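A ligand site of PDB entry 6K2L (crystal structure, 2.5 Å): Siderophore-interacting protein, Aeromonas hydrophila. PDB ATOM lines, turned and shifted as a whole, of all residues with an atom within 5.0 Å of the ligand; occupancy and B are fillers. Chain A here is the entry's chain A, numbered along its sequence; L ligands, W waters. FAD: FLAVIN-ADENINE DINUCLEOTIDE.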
ATOM      1  N   HIS A  46      14.714  -5.383 -30.698  1.00  0.00           N
ATOM      2  CA  HIS A  46      15.770  -4.488 -30.290  1.00  0.00           C
ATOM      3  C   HIS A  46      15.934  -3.373 -31.299  1.00  0.00           C
ATOM      4  O   HIS A  46      15.617  -3.521 -32.479  1.00  0.00           O
ATOM      5  CB  HIS A  46      17.102  -5.218 -30.154  1.00  0.00           C
ATOM      6  CG  HIS A  46      16.953  -6.555 -29.508  1.00  0.00           C
ATOM      7  ND1 HIS A  46      17.768  -7.623 -29.808  1.00  0.00           N
ATOM      8  CD2 HIS A  46      16.081  -6.989 -28.577  1.00  0.00           C
ATOM      9  CE1 HIS A  46      17.404  -8.663 -29.078  1.00  0.00           C
ATOM     10  NE2 HIS A  46      16.379  -8.305 -28.319  1.00  0.00           N
ATOM     11  N   ARG A  81      23.115   3.083 -27.826  1.00  0.00           N
ATOM     12  CA  ARG A  81      22.671   2.165 -26.783  1.00  0.00           C
ATOM     13  C   ARG A  81      21.612   1.238 -27.362  1.00  0.00           C
ATOM     14  O   ARG A  81      20.853   1.644 -28.245  1.00  0.00           O
ATOM     15  CB  ARG A  81      22.077   2.904 -25.562  1.00  0.00           C
ATOM     16  CG  ARG A  81      23.074   3.791 -24.811  1.00  0.00           C
ATOM     17  CD  ARG A  81      24.077   2.962 -24.091  1.00  0.00           C
ATOM     18  NE  ARG A  81      24.957   3.726 -23.204  1.00  0.00           N
ATOM     19  CZ  ARG A  81      26.183   4.155 -23.555  1.00  0.00           C
ATOM     20  NH1 ARG A  81      26.619   3.937 -24.782  1.00  0.00           N
ATOM     21  NH2 ARG A  81      26.959   4.781 -22.686  1.00  0.00           N
ATOM     22  N   THR A  82      21.541   0.025 -26.839  1.00  0.00           N
ATOM     23  CA  THR A  82      20.529  -0.936 -27.261  1.00  0.00           C
ATOM     24  C   THR A  82      19.296  -0.844 -26.365  1.00  0.00           C
ATOM     25  O   THR A  82      19.420  -0.820 -25.139  1.00  0.00           O
ATOM     26  CB  THR A  82      21.076  -2.355 -27.245  1.00  0.00           C
ATOM     27  OG1 THR A  82      22.243  -2.387 -28.067  1.00  0.00           O
ATOM     28  CG2 THR A  82      20.025  -3.324 -27.812  1.00  0.00           C
ATOM     29  N   PHE A  83      18.108  -0.818 -26.974  1.00  0.00           N
ATOM     30  CA  PHE A  83      16.864  -0.753 -26.227  1.00  0.00           C
ATOM     31  C   PHE A  83      15.820  -1.591 -26.935  1.00  0.00           C
ATOM     32  O   PHE A  83      16.006  -2.037 -28.060  1.00  0.00           O
ATOM     33  CB  PHE A  83      16.367   0.697 -26.027  1.00  0.00           C
ATOM     34  CG  PHE A  83      17.060   1.401 -24.881  1.00  0.00           C
ATOM     35  CD1 PHE A  83      18.326   1.928 -25.058  1.00  0.00           C
ATOM     36  CD2 PHE A  83      16.458   1.480 -23.649  1.00  0.00           C
ATOM     37  CE1 PHE A  83      18.967   2.523 -24.035  1.00  0.00           C
ATOM     38  CE2 PHE A  83      17.105   2.054 -22.606  1.00  0.00           C
ATOM     39  CZ  PHE A  83      18.374   2.584 -22.805  1.00  0.00           C
ATOM     40  N   THR A  84      14.720  -1.820 -26.241  1.00  0.00           N
ATOM     41  CA  THR A  84      13.644  -2.651 -26.709  1.00  0.00           C
ATOM     42  C   THR A  84      12.515  -1.745 -27.168  1.00  0.00           C
ATOM     43  O   THR A  84      12.205  -0.762 -26.496  1.00  0.00           O
ATOM     44  CB  THR A  84      13.172  -3.538 -25.554  1.00  0.00           C
ATOM     45  OG1 THR A  84      14.290  -4.291 -25.083  1.00  0.00           O
ATOM     46  CG2 THR A  84      11.993  -4.477 -25.975  1.00  0.00           C
ATOM     47  N   ASP A  98      10.692   1.779 -22.993  1.00  0.00           N
ATOM     48  CA  ASP A  98      10.687   1.824 -21.521  1.00  0.00           C
ATOM     49  C   ASP A  98      12.107   1.827 -20.949  1.00  0.00           C
ATOM     50  O   ASP A  98      12.862   0.863 -21.125  1.00  0.00           O
ATOM     51  CB  ASP A  98       9.930   0.636 -20.940  1.00  0.00           C
ATOM     52  CG  ASP A  98       8.429   0.673 -21.186  1.00  0.00           C
ATOM     53  OD1 ASP A  98       7.897   1.658 -21.753  1.00  0.00           O
ATOM     54  OD2 ASP A  98       7.772  -0.327 -20.786  1.00  0.00           O
ATOM     55  N   PHE A  99      12.442   2.886 -20.198  1.00  0.00           N
ATOM     56  CA  PHE A  99      13.766   3.112 -19.639  1.00  0.00           C
ATOM     57  C   PHE A  99      13.823   2.674 -18.170  1.00  0.00           C
ATOM     58  O   PHE A  99      13.032   3.168 -17.347  1.00  0.00           O
ATOM     59  CB  PHE A  99      14.139   4.605 -19.756  1.00  0.00           C
ATOM     60  CG  PHE A  99      14.559   5.001 -21.133  1.00  0.00           C
ATOM     61  CD1 PHE A  99      13.610   5.164 -22.151  1.00  0.00           C
ATOM     62  CD2 PHE A  99      15.906   5.183 -21.441  1.00  0.00           C
ATOM     63  CE1 PHE A  99      13.997   5.510 -23.432  1.00  0.00           C
ATOM     64  CE2 PHE A  99      16.291   5.529 -22.736  1.00  0.00           C
ATOM     65  CZ  PHE A  99      15.342   5.700 -23.725  1.00  0.00           C
ATOM     66  N   ALA A 100      14.761   1.776 -17.834  1.00  0.00           N
ATOM     67  CA  ALA A 100      15.017   1.420 -16.426  1.00  0.00           C
ATOM     68  C   ALA A 100      15.825   2.557 -15.788  1.00  0.00           C
ATOM     69  O   ALA A 100      17.032   2.663 -15.992  1.00  0.00           O
ATOM     70  CB  ALA A 100      15.745   0.093 -16.312  1.00  0.00           C
ATOM     71  N   LEU A 101      15.146   3.405 -15.010  1.00  0.00           N
ATOM     72  CA  LEU A 101      15.786   4.564 -14.370  1.00  0.00           C
ATOM     73  C   LEU A 101      16.851   4.134 -13.373  1.00  0.00           C
ATOM     74  O   LEU A 101      16.699   3.134 -12.663  1.00  0.00           O
ATOM     75  CB  LEU A 101      14.719   5.419 -13.654  1.00  0.00           C
ATOM     76  CG  LEU A 101      13.667   6.175 -14.505  1.00  0.00           C
ATOM     77  CD1 LEU A 101      12.833   7.137 -13.662  1.00  0.00           C
ATOM     78  CD2 LEU A 101      14.286   6.907 -15.711  1.00  0.00           C
ATOM     79  N   HIS A 102      17.967   4.868 -13.347  1.00  0.00           N
ATOM     80  CA  HIS A 102      19.059   4.653 -12.399  1.00  0.00           C
ATOM     81  C   HIS A 102      19.813   5.966 -12.243  1.00  0.00           C
ATOM     82  O   HIS A 102      19.517   6.976 -12.899  1.00  0.00           O
ATOM     83  CB  HIS A 102      20.008   3.522 -12.833  1.00  0.00           C
ATOM     84  CG  HIS A 102      20.732   3.792 -14.118  1.00  0.00           C
ATOM     85  ND1 HIS A 102      22.037   4.236 -14.165  1.00  0.00           N
ATOM     86  CD2 HIS A 102      20.327   3.687 -15.414  1.00  0.00           C
ATOM     87  CE1 HIS A 102      22.408   4.387 -15.419  1.00  0.00           C
ATOM     88  NE2 HIS A 102      21.387   4.052 -16.200  1.00  0.00           N
ATOM     89  N   ASP A 104      23.537   5.961 -11.997  1.00  0.00           N
ATOM     90  CA  ASP A 104      24.943   5.710 -12.235  1.00  0.00           C
ATOM     91  C   ASP A 104      25.466   6.427 -13.485  1.00  0.00           C
ATOM     92  O   ASP A 104      26.609   6.171 -13.887  1.00  0.00           O
ATOM     93  CB  ASP A 104      25.219   4.196 -12.327  1.00  0.00           C
ATOM     94  CG  ASP A 104      24.862   3.441 -11.036  1.00  0.00           C
ATOM     95  OD1 ASP A 104      24.000   2.516 -11.071  1.00  0.00           O
ATOM     96  OD2 ASP A 104      25.425   3.793  -9.971  1.00  0.00           O
ATOM     97  N   GLY A 105      24.651   7.294 -14.102  1.00  0.00           N
ATOM     98  CA  GLY A 105      25.100   8.097 -15.233  1.00  0.00           C
ATOM     99  C   GLY A 105      25.152   7.353 -16.559  1.00  0.00           C
ATOM    100  O   GLY A 105      24.864   6.156 -16.648  1.00  0.00           O
ATOM    101  N   GLY A 106      25.515   8.078 -17.616  1.00  0.00           N
ATOM    102  CA  GLY A 106      25.497   7.551 -18.979  1.00  0.00           C
ATOM    103  C   GLY A 106      24.533   8.335 -19.848  1.00  0.00           C
ATOM    104  O   GLY A 106      23.582   8.941 -19.338  1.00  0.00           O
ATOM    105  N   PRO A 107      24.765   8.357 -21.164  1.00  0.00           N
ATOM    106  CA  PRO A 107      23.905   9.187 -22.032  1.00  0.00           C
ATOM    107  C   PRO A 107      22.443   8.776 -22.049  1.00  0.00           C
ATOM    108  O   PRO A 107      21.574   9.650 -22.080  1.00  0.00           O
ATOM    109  CB  PRO A 107      24.555   9.034 -23.422  1.00  0.00           C
ATOM    110  CG  PRO A 107      25.271   7.729 -23.370  1.00  0.00           C
ATOM    111  CD  PRO A 107      25.772   7.623 -21.941  1.00  0.00           C
ATOM    112  N   ALA A 108      22.129   7.479 -22.086  1.00  0.00           N
ATOM    113  CA  ALA A 108      20.713   7.084 -22.115  1.00  0.00           C
ATOM    114  C   ALA A 108      20.015   7.423 -20.801  1.00  0.00           C
ATOM    115  O   ALA A 108      18.857   7.859 -20.816  1.00  0.00           O
ATOM    116  CB  ALA A 108      20.564   5.594 -22.428  1.00  0.00           C
ATOM    117  N   SER A 109      20.706   7.233 -19.671  1.00  0.00           N
ATOM    118  CA  SER A 109      20.147   7.651 -18.382  1.00  0.00           C
ATOM    119  C   SER A 109      19.852   9.139 -18.366  1.00  0.00           C
ATOM    120  O   SER A 109      18.819   9.548 -17.834  1.00  0.00           O
ATOM    121  CB  SER A 109      21.105   7.298 -17.240  1.00  0.00           C
ATOM    122  OG  SER A 109      20.515   7.646 -15.991  1.00  0.00           O
ATOM    123  N   THR A 146      15.749  -3.961 -16.911  1.00  0.00           N
ATOM    124  CA  THR A 146      16.137  -3.709 -18.287  1.00  0.00           C
ATOM    125  C   THR A 146      15.536  -4.711 -19.265  1.00  0.00           C
ATOM    126  O   THR A 146      15.405  -4.398 -20.455  1.00  0.00           O
ATOM    127  CB  THR A 146      17.657  -3.722 -18.428  1.00  0.00           C
ATOM    128  OG1 THR A 146      18.136  -5.049 -18.209  1.00  0.00           O
ATOM    129  CG2 THR A 146      18.285  -2.810 -17.434  1.00  0.00           C
ATOM    130  N   PRO A 149      10.682  -4.673 -20.220  1.00  0.00           N
ATOM    131  CA  PRO A 149       9.895  -4.267 -21.391  1.00  0.00           C
ATOM    132  C   PRO A 149       9.773  -5.351 -22.450  1.00  0.00           C
ATOM    133  O   PRO A 149       8.676  -5.568 -22.983  1.00  0.00           O
ATOM    134  CB  PRO A 149      10.620  -3.015 -21.874  1.00  0.00           C
ATOM    135  CG  PRO A 149      11.273  -2.484 -20.590  1.00  0.00           C
ATOM    136  CD  PRO A 149      11.735  -3.691 -19.903  1.00  0.00           C
ATOM    137  N   TYR A 244      17.580 -18.204 -25.449  1.00  0.00           N
ATOM    138  CA  TYR A 244      18.021 -16.829 -25.614  1.00  0.00           C
ATOM    139  C   TYR A 244      18.758 -16.458 -24.322  1.00  0.00           C
ATOM    140  O   TYR A 244      18.201 -16.572 -23.214  1.00  0.00           O
ATOM    141  CB  TYR A 244      16.808 -15.939 -25.905  1.00  0.00           C
ATOM    142  CG  TYR A 244      17.049 -14.445 -25.954  1.00  0.00           C
ATOM    143  CD1 TYR A 244      17.194 -13.692 -24.776  1.00  0.00           C
ATOM    144  CD2 TYR A 244      17.056 -13.777 -27.171  1.00  0.00           C
ATOM    145  CE1 TYR A 244      17.376 -12.311 -24.827  1.00  0.00           C
ATOM    146  CE2 TYR A 244      17.247 -12.400 -27.244  1.00  0.00           C
ATOM    147  CZ  TYR A 244      17.406 -11.674 -26.069  1.00  0.00           C
ATOM    148  OH  TYR A 244      17.585 -10.305 -26.140  1.00  0.00           O
ATOM    149  N   VAL A 246      21.162 -13.282 -23.443  1.00  0.00           N
ATOM    150  CA  VAL A 246      21.790 -12.033 -23.863  1.00  0.00           C
ATOM    151  C   VAL A 246      21.916 -11.172 -22.609  1.00  0.00           C
ATOM    152  O   VAL A 246      20.893 -10.772 -22.036  1.00  0.00           O
ATOM    153  CB  VAL A 246      20.957 -11.307 -24.930  1.00  0.00           C
ATOM    154  CG1 VAL A 246      21.558  -9.968 -25.223  1.00  0.00           C
ATOM    155  CG2 VAL A 246      20.836 -12.131 -26.177  1.00  0.00           C
ATOM    156  N   PRO A 247      23.125 -10.863 -22.140  1.00  0.00           N
ATOM    157  CA  PRO A 247      23.248  -9.948 -20.991  1.00  0.00           C
ATOM    158  C   PRO A 247      23.007  -8.522 -21.469  1.00  0.00           C
ATOM    159  O   PRO A 247      23.661  -8.049 -22.399  1.00  0.00           O
ATOM    160  CB  PRO A 247      24.677 -10.163 -20.489  1.00  0.00           C
ATOM    161  CG  PRO A 247      25.252 -11.312 -21.372  1.00  0.00           C
ATOM    162  CD  PRO A 247      24.440 -11.338 -22.618  1.00  0.00           C
ATOM    163  N   TYR A 248      22.028  -7.860 -20.861  1.00  0.00           N
ATOM    164  CA  TYR A 248      21.652  -6.523 -21.315  1.00  0.00           C
ATOM    165  C   TYR A 248      22.638  -5.469 -20.817  1.00  0.00           C
ATOM    166  O   TYR A 248      22.810  -4.451 -21.479  1.00  0.00           O
ATOM    167  CB  TYR A 248      20.233  -6.185 -20.854  1.00  0.00           C
ATOM    168  CG  TYR A 248      19.131  -6.774 -21.742  1.00  0.00           C
ATOM    169  CD1 TYR A 248      19.408  -7.801 -22.625  1.00  0.00           C
ATOM    170  CD2 TYR A 248      17.825  -6.302 -21.672  1.00  0.00           C
ATOM    171  CE1 TYR A 248      18.419  -8.324 -23.421  1.00  0.00           C
ATOM    172  CE2 TYR A 248      16.841  -6.821 -22.475  1.00  0.00           C
ATOM    173  CZ  TYR A 248      17.134  -7.818 -23.346  1.00  0.00           C
ATOM    174  OH  TYR A 248      16.154  -8.345 -24.164  1.00  0.00           O
ATOM    175  N   TRP A 249      23.285  -5.709 -19.674  1.00  0.00           N
ATOM    176  CA  TRP A 249      24.287  -4.813 -19.109  1.00  0.00           C
ATOM    177  C   TRP A 249      25.051  -5.556 -18.019  1.00  0.00           C
ATOM    178  O   TRP A 249      24.773  -6.727 -17.716  1.00  0.00           O
ATOM    179  CB  TRP A 249      23.671  -3.544 -18.532  1.00  0.00           C
ATOM    180  CG  TRP A 249      22.747  -3.777 -17.362  1.00  0.00           C
ATOM    181  CD1 TRP A 249      21.541  -4.423 -17.382  1.00  0.00           C
ATOM    182  CD2 TRP A 249      22.952  -3.363 -16.005  1.00  0.00           C
ATOM    183  NE1 TRP A 249      20.981  -4.427 -16.121  1.00  0.00           N
ATOM    184  CE2 TRP A 249      21.823  -3.774 -15.260  1.00  0.00           C
ATOM    185  CE3 TRP A 249      23.976  -2.671 -15.340  1.00  0.00           C
ATOM    186  CZ2 TRP A 249      21.689  -3.539 -13.889  1.00  0.00           C
ATOM    187  CZ3 TRP A 249      23.847  -2.433 -13.977  1.00  0.00           C
ATOM    188  CH2 TRP A 249      22.712  -2.855 -13.267  1.00  0.00           C
ATOM    189  N   ARG A 250      26.019  -4.866 -17.417  1.00  0.00           N
ATOM    190  CA  ARG A 250      26.859  -5.470 -16.392  1.00  0.00           C
ATOM    191  C   ARG A 250      27.079  -4.437 -15.305  1.00  0.00           C
ATOM    192  O   ARG A 250      27.570  -3.334 -15.588  1.00  0.00           O
ATOM    193  CB  ARG A 250      28.182  -5.941 -16.979  1.00  0.00           C
ATOM    194  CG  ARG A 250      29.029  -6.677 -15.972  1.00  0.00           C
ATOM    195  CD  ARG A 250      30.120  -7.477 -16.647  1.00  0.00           C
ATOM    196  NE  ARG A 250      30.984  -8.185 -15.706  1.00  0.00           N
ATOM    197  CZ  ARG A 250      32.099  -8.829 -16.060  1.00  0.00           C
ATOM    198  NH1 ARG A 250      32.487  -8.840 -17.326  1.00  0.00           N
ATOM    199  NH2 ARG A 250      32.836  -9.446 -15.136  1.00  0.00           N
ATOM    200  N   HIS A 251      26.679  -4.774 -14.079  1.00  0.00           N
ATOM    201  CA  HIS A 251      26.857  -3.922 -12.911  1.00  0.00           C
ATOM    202  C   HIS A 251      28.267  -3.337 -12.849  1.00  0.00           C
ATOM    203  O   HIS A 251      29.252  -4.075 -12.845  1.00  0.00           O
ATOM    204  CB  HIS A 251      26.556  -4.744 -11.664  1.00  0.00           C
ATOM    205  CG  HIS A 251      26.519  -3.953 -10.396  1.00  0.00           C
ATOM    206  ND1 HIS A 251      26.251  -2.599 -10.372  1.00  0.00           N
ATOM    207  CD2 HIS A 251      26.704  -4.325  -9.108  1.00  0.00           C
ATOM    208  CE1 HIS A 251      26.262  -2.170  -9.125  1.00  0.00           C
ATOM    209  NE2 HIS A 251      26.533  -3.206  -8.330  1.00  0.00           N
ATOM    210  N   GLY A 252      28.335  -2.002 -12.842  1.00  0.00           N
ATOM    211  CA  GLY A 252      29.593  -1.279 -12.714  1.00  0.00           C
ATOM    212  C   GLY A 252      30.335  -0.999 -14.009  1.00  0.00           C
ATOM    213  O   GLY A 252      31.444  -0.465 -13.964  1.00  0.00           O
ATOM    214  N   LYS A 253      29.787  -1.369 -15.161  1.00  0.00           N
ATOM    215  CA  LYS A 253      30.467  -1.160 -16.427  1.00  0.00           C
ATOM    216  C   LYS A 253      29.520  -0.419 -17.357  1.00  0.00           C
ATOM    217  O   LYS A 253      28.357  -0.811 -17.513  1.00  0.00           O
ATOM    218  CB  LYS A 253      30.923  -2.478 -17.068  1.00  0.00           C
ATOM    219  CG  LYS A 253      31.736  -3.361 -16.152  1.00  0.00           C
ATOM    220  CD  LYS A 253      32.906  -3.993 -16.928  1.00  0.00           C
ATOM    221  CE  LYS A 253      32.367  -4.778 -18.139  1.00  0.00           C
ATOM    222  NZ  LYS A 253      33.308  -4.835 -19.302  1.00  0.00           N
ATOM    223  N   ASP A 254      30.013   0.669 -17.954  1.00  0.00           N
ATOM    224  CA  ASP A 254      29.229   1.316 -18.986  1.00  0.00           C
ATOM    225  C   ASP A 254      29.265   0.479 -20.275  1.00  0.00           C
ATOM    226  O   ASP A 254      30.043  -0.487 -20.412  1.00  0.00           O
ATOM    227  CB  ASP A 254      29.743   2.737 -19.209  1.00  0.00           C
ATOM    228  CG  ASP A 254      31.270   2.805 -19.321  1.00  0.00           C
ATOM    229  OD1 ASP A 254      31.841   2.187 -20.244  1.00  0.00           O
ATOM    230  OD2 ASP A 254      31.912   3.475 -18.469  1.00  0.00           O
ATOM    231  N   GLU A 255      28.384   0.845 -21.206  1.00  0.00           N
ATOM    232  CA  GLU A 255      28.294   0.132 -22.484  1.00  0.00           C
ATOM    233  C   GLU A 255      29.626   0.152 -23.249  1.00  0.00           C
ATOM    234  O   GLU A 255      29.925  -0.783 -23.998  1.00  0.00           O
ATOM    235  CB  GLU A 255      27.182   0.750 -23.322  1.00  0.00           C
ATOM    236  CG  GLU A 255      27.187   0.303 -24.786  1.00  0.00           C
ATOM    237  CD  GLU A 255      26.838  -1.187 -24.936  1.00  0.00           C
ATOM    238  OE1 GLU A 255      26.070  -1.705 -24.077  1.00  0.00           O
ATOM    239  OE2 GLU A 255      27.319  -1.816 -25.911  1.00  0.00           O
ATOM    240  N   ARG A 262      30.308  -8.330 -23.902  1.00  0.00           N
ATOM    241  CA  ARG A 262      28.980  -8.910 -24.140  1.00  0.00           C
ATOM    242  C   ARG A 262      28.997  -9.786 -25.370  1.00  0.00           C
ATOM    243  O   ARG A 262      28.384 -10.871 -25.392  1.00  0.00           O
ATOM    244  CB  ARG A 262      27.913  -7.814 -24.290  1.00  0.00           C
ATOM    245  CG  ARG A 262      26.461  -8.325 -24.153  1.00  0.00           C
ATOM    246  CD  ARG A 262      25.470  -7.472 -24.931  1.00  0.00           C
ATOM    247  NE  ARG A 262      24.933  -6.340 -24.147  1.00  0.00           N
ATOM    248  CZ  ARG A 262      25.359  -5.071 -24.254  1.00  0.00           C
ATOM    249  NH1 ARG A 262      26.344  -4.788 -25.103  1.00  0.00           N
ATOM    250  NH2 ARG A 262      24.806  -4.105 -23.506  1.00  0.00           N
HETATM  251  PA  FAD L   1      25.768   3.371 -19.331  1.00  0.00           P
HETATM  252  O1A FAD L   1      26.391   4.638 -19.836  1.00  0.00           O
HETATM  253  O2A FAD L   1      25.847   2.171 -20.283  1.00  0.00           O
HETATM  254  O5B FAD L   1      26.407   2.807 -17.957  1.00  0.00           O
HETATM  255  C5B FAD L   1      26.635   3.666 -16.817  1.00  0.00           C
HETATM  256  C4B FAD L   1      26.709   2.887 -15.520  1.00  0.00           C
HETATM  257  O4B FAD L   1      25.375   2.572 -15.060  1.00  0.00           O
HETATM  258  C3B FAD L   1      27.466   1.565 -15.538  1.00  0.00           C
HETATM  259  O3B FAD L   1      28.132   1.360 -14.290  1.00  0.00           O
HETATM  260  C2B FAD L   1      26.346   0.536 -15.755  1.00  0.00           C
HETATM  261  O2B FAD L   1      26.606  -0.769 -15.234  1.00  0.00           O
HETATM  262  C1B FAD L   1      25.194   1.166 -14.981  1.00  0.00           C
HETATM  263  N9A FAD L   1      23.906   0.883 -15.568  1.00  0.00           N
HETATM  264  C8A FAD L   1      23.588   0.875 -16.903  1.00  0.00           C
HETATM  265  N7A FAD L   1      22.327   0.621 -17.150  1.00  0.00           N
HETATM  266  C5A FAD L   1      21.764   0.478 -15.892  1.00  0.00           C
HETATM  267  C6A FAD L   1      20.453   0.202 -15.463  1.00  0.00           C
HETATM  268  N6A FAD L   1      19.428   0.064 -16.297  1.00  0.00           N
HETATM  269  N1A FAD L   1      20.240   0.108 -14.129  1.00  0.00           N
HETATM  270  C2A FAD L   1      21.267   0.270 -13.295  1.00  0.00           C
HETATM  271  N3A FAD L   1      22.556   0.544 -13.586  1.00  0.00           N
HETATM  272  C4A FAD L   1      22.730   0.637 -14.907  1.00  0.00           C
HETATM  273  N1  FAD L   1      17.683  -1.131 -20.956  1.00  0.00           N
HETATM  274  C2  FAD L   1      16.510  -0.489 -20.679  1.00  0.00           C
HETATM  275  O2  FAD L   1      16.408   0.335 -19.773  1.00  0.00           O
HETATM  276  N3  FAD L   1      15.377  -0.763 -21.430  1.00  0.00           N
HETATM  277  C4  FAD L   1      15.294  -1.654 -22.476  1.00  0.00           C
HETATM  278  O4  FAD L   1      14.224  -1.804 -23.076  1.00  0.00           O
HETATM  279  C4X FAD L   1      16.548  -2.316 -22.786  1.00  0.00           C
HETATM  280  N5  FAD L   1      16.568  -3.189 -23.781  1.00  0.00           N
HETATM  281  C5X FAD L   1      17.760  -3.821 -24.053  1.00  0.00           C
HETATM  282  C6  FAD L   1      17.785  -4.756 -25.086  1.00  0.00           C
HETATM  283  C7  FAD L   1      18.962  -5.439 -25.393  1.00  0.00           C
HETATM  284  C7M FAD L   1      18.955  -6.427 -26.537  1.00  0.00           C
HETATM  285  C8  FAD L   1      20.137  -5.173 -24.669  1.00  0.00           C
HETATM  286  C8M FAD L   1      21.438  -5.865 -25.000  1.00  0.00           C
HETATM  287  C9  FAD L   1      20.112  -4.226 -23.643  1.00  0.00           C
HETATM  288  C9A FAD L   1      18.935  -3.555 -23.330  1.00  0.00           C
HETATM  289  N10 FAD L   1      18.877  -2.629 -22.271  1.00  0.00           N
HETATM  290  C10 FAD L   1      17.690  -1.998 -21.957  1.00  0.00           C
HETATM  291  C1' FAD L   1      20.071  -2.349 -21.464  1.00  0.00           C
HETATM  292  C2' FAD L   1      20.681  -0.967 -21.680  1.00  0.00           C
HETATM  293  O2' FAD L   1      21.325  -0.869 -22.957  1.00  0.00           O
HETATM  294  C3' FAD L   1      21.694  -0.689 -20.570  1.00  0.00           C
HETATM  295  O3' FAD L   1      20.977  -0.443 -19.363  1.00  0.00           O
HETATM  296  C4' FAD L   1      22.638   0.482 -20.842  1.00  0.00           C
HETATM  297  O4' FAD L   1      23.830   0.282 -20.079  1.00  0.00           O
HETATM  298  C5' FAD L   1      21.988   1.800 -20.510  1.00  0.00           C
HETATM  299  O5' FAD L   1      22.848   2.870 -20.936  1.00  0.00           O
HETATM  300  P   FAD L   1      23.115   4.128 -20.022  1.00  0.00           P
HETATM  301  O1P FAD L   1      23.737   5.191 -20.944  1.00  0.00           O
HETATM  302  O2P FAD L   1      21.924   4.556 -19.290  1.00  0.00           O
HETATM  303  O3P FAD L   1      24.239   3.614 -18.999  1.00  0.00           O
HETATM  304  O   HOH W   1      19.082   1.007 -18.767  1.00  0.00           O
HETATM  305  O   HOH W   2      11.859  -0.780 -24.044  1.00  0.00           O
HETATM  306  O   HOH W   3      13.697  -4.998 -22.382  1.00  0.00           O
HETATM  307  O   HOH W   4      25.695  -1.980 -21.134  1.00  0.00           O
HETATM  308  O   HOH W   5      19.314   3.702 -19.308  1.00  0.00           O
HETATM  309  O   HOH W   6      23.548  -0.514 -24.700  1.00  0.00           O
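Water W2 lies within hydrogen-bond range of the backbone carbonyl oxygen of Thr 84 (2.5 Å), an oxygen (O4) of the ligand (2.8 Å) and the backbone NH of Asp 98 (3.0 Å). Water W6 lies within hydrogen-bond range of O2' of the ligand (2.8 Å), OE1 of Glu 255 (2.9 Å) and N of Thr 82 (3.0 Å). Water W4 lies within hydrogen-bond range of the side-chain carboxylate of Glu 255 (3.0 Å), an oxygen (O4') of the ligand (3.1 Å) and the guanidinium group of Arg 262 (3.3 Å). Water W3 lies within hydrogen-bond range of the backbone carbonyl oxygen (O) of Thr 146 (2.6 Å), the side-chain hydroxyl (OG1) of Thr 84 (2.9 Å) and an oxygen (O4) of the ligand (3.3 Å).
OH of Tyr 248 sits at hydrogen-bond distance from OH of Tyr 244. The guanidinium group of Arg 262 sits at hydrogen-bond distance from the backbone carbonyl oxygen of Pro 247 (2.8 Å). A ring nitrogen (NE2) of His 46 is in hydrogen-bond range of the side-chain hydroxyl (OH) of Tyr 244 (3.2 Å). ND1 of His 102 sits at hydrogen-bond distance from N of Asp 104 (3.2 Å). The backbone carbonyl oxygen (O) of His 102 sits at hydrogen-bond distance from the side-chain hydroxyl (OG) of Ser 109 (3.3 Å). The guanidinium group of Arg 262 lies within salt-bridge range of the side-chain carboxylate of Glu 255 (2.8 Å). The guanidinium group (NH2) of Arg 262 is in hydrogen-bond range of the backbone carbonyl oxygen (O) of Tyr 248 (2.9 Å).
The backbone nitrogen (N) of Pro 107 sits close to an oxygen (O1P) of the ligand, 3.3 Å away. Residues that only touch the ligand: His 46, Phe 83, Phe 99, Asp 104, Gly 105, Gly 106, Thr 146, Pro 149, Tyr 248, Trp 249, His 251, Asp 254 and Arg 262. Hydrophobic or aromatic side chains that line the ligand: His 46, Phe 83, Ala 100, His 102, Pro 107, Ala 108, Pro 149, Tyr 248 and Trp 249. The nearest printed residue that does not touch the ligand is Pro 247 (4.1 Å).
A ring nitrogen (NE2) of His 102 sits at hydrogen-bond distance from an oxygen (O2P) of the ligand (3.2 Å). An oxygen (O2P) of the ligand sits at hydrogen-bond distance from the backbone NH (N) of Ser 109 (3.0 Å). N of Thr 84 lies close to O4 of the ligand, 3.2 Å away. O of Arg 250 sits at hydrogen-bond distance from O2B of the ligand. The backbone NH of Ala 100 lies within hydrogen-bond range of an oxygen (O2) of the ligand (2.9 Å). N5 of the ligand is in hydrogen-bond range of OG1 of Thr 84 (2.8 Å). The backbone NH (N) of Gly 252 lies within hydrogen-bond range of an oxygen (O2B) of the ligand (3.2 Å). An oxygen (O2A) of the ligand lies within hydrogen-bond range of the backbone NH (N) of Glu 255, at 3.0 Å. The backbone NH (N) of Lys 253 is in hydrogen-bond range of an oxygen (O2B) of the ligand, 3.2 Å away. The backbone carbonyl oxygen (O) of Thr 82 sits at hydrogen-bond distance from an oxygen (O2') of the ligand (2.9 Å). The backbone carbonyl oxygen of Asp 98 is in hydrogen-bond range of a nitrogen (N3) of the ligand (3.0 Å). The backbone NH (N) of Ala 108 sits at hydrogen-bond distance from an oxygen (O1P) of the ligand (3.0 Å). The backbone carbonyl oxygen of Lys 253 sits at hydrogen-bond distance from an oxygen (O2B) of the ligand, at 2.9 Å. O1A of the ligand lies within salt-bridge range of NH2 of Arg 81.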
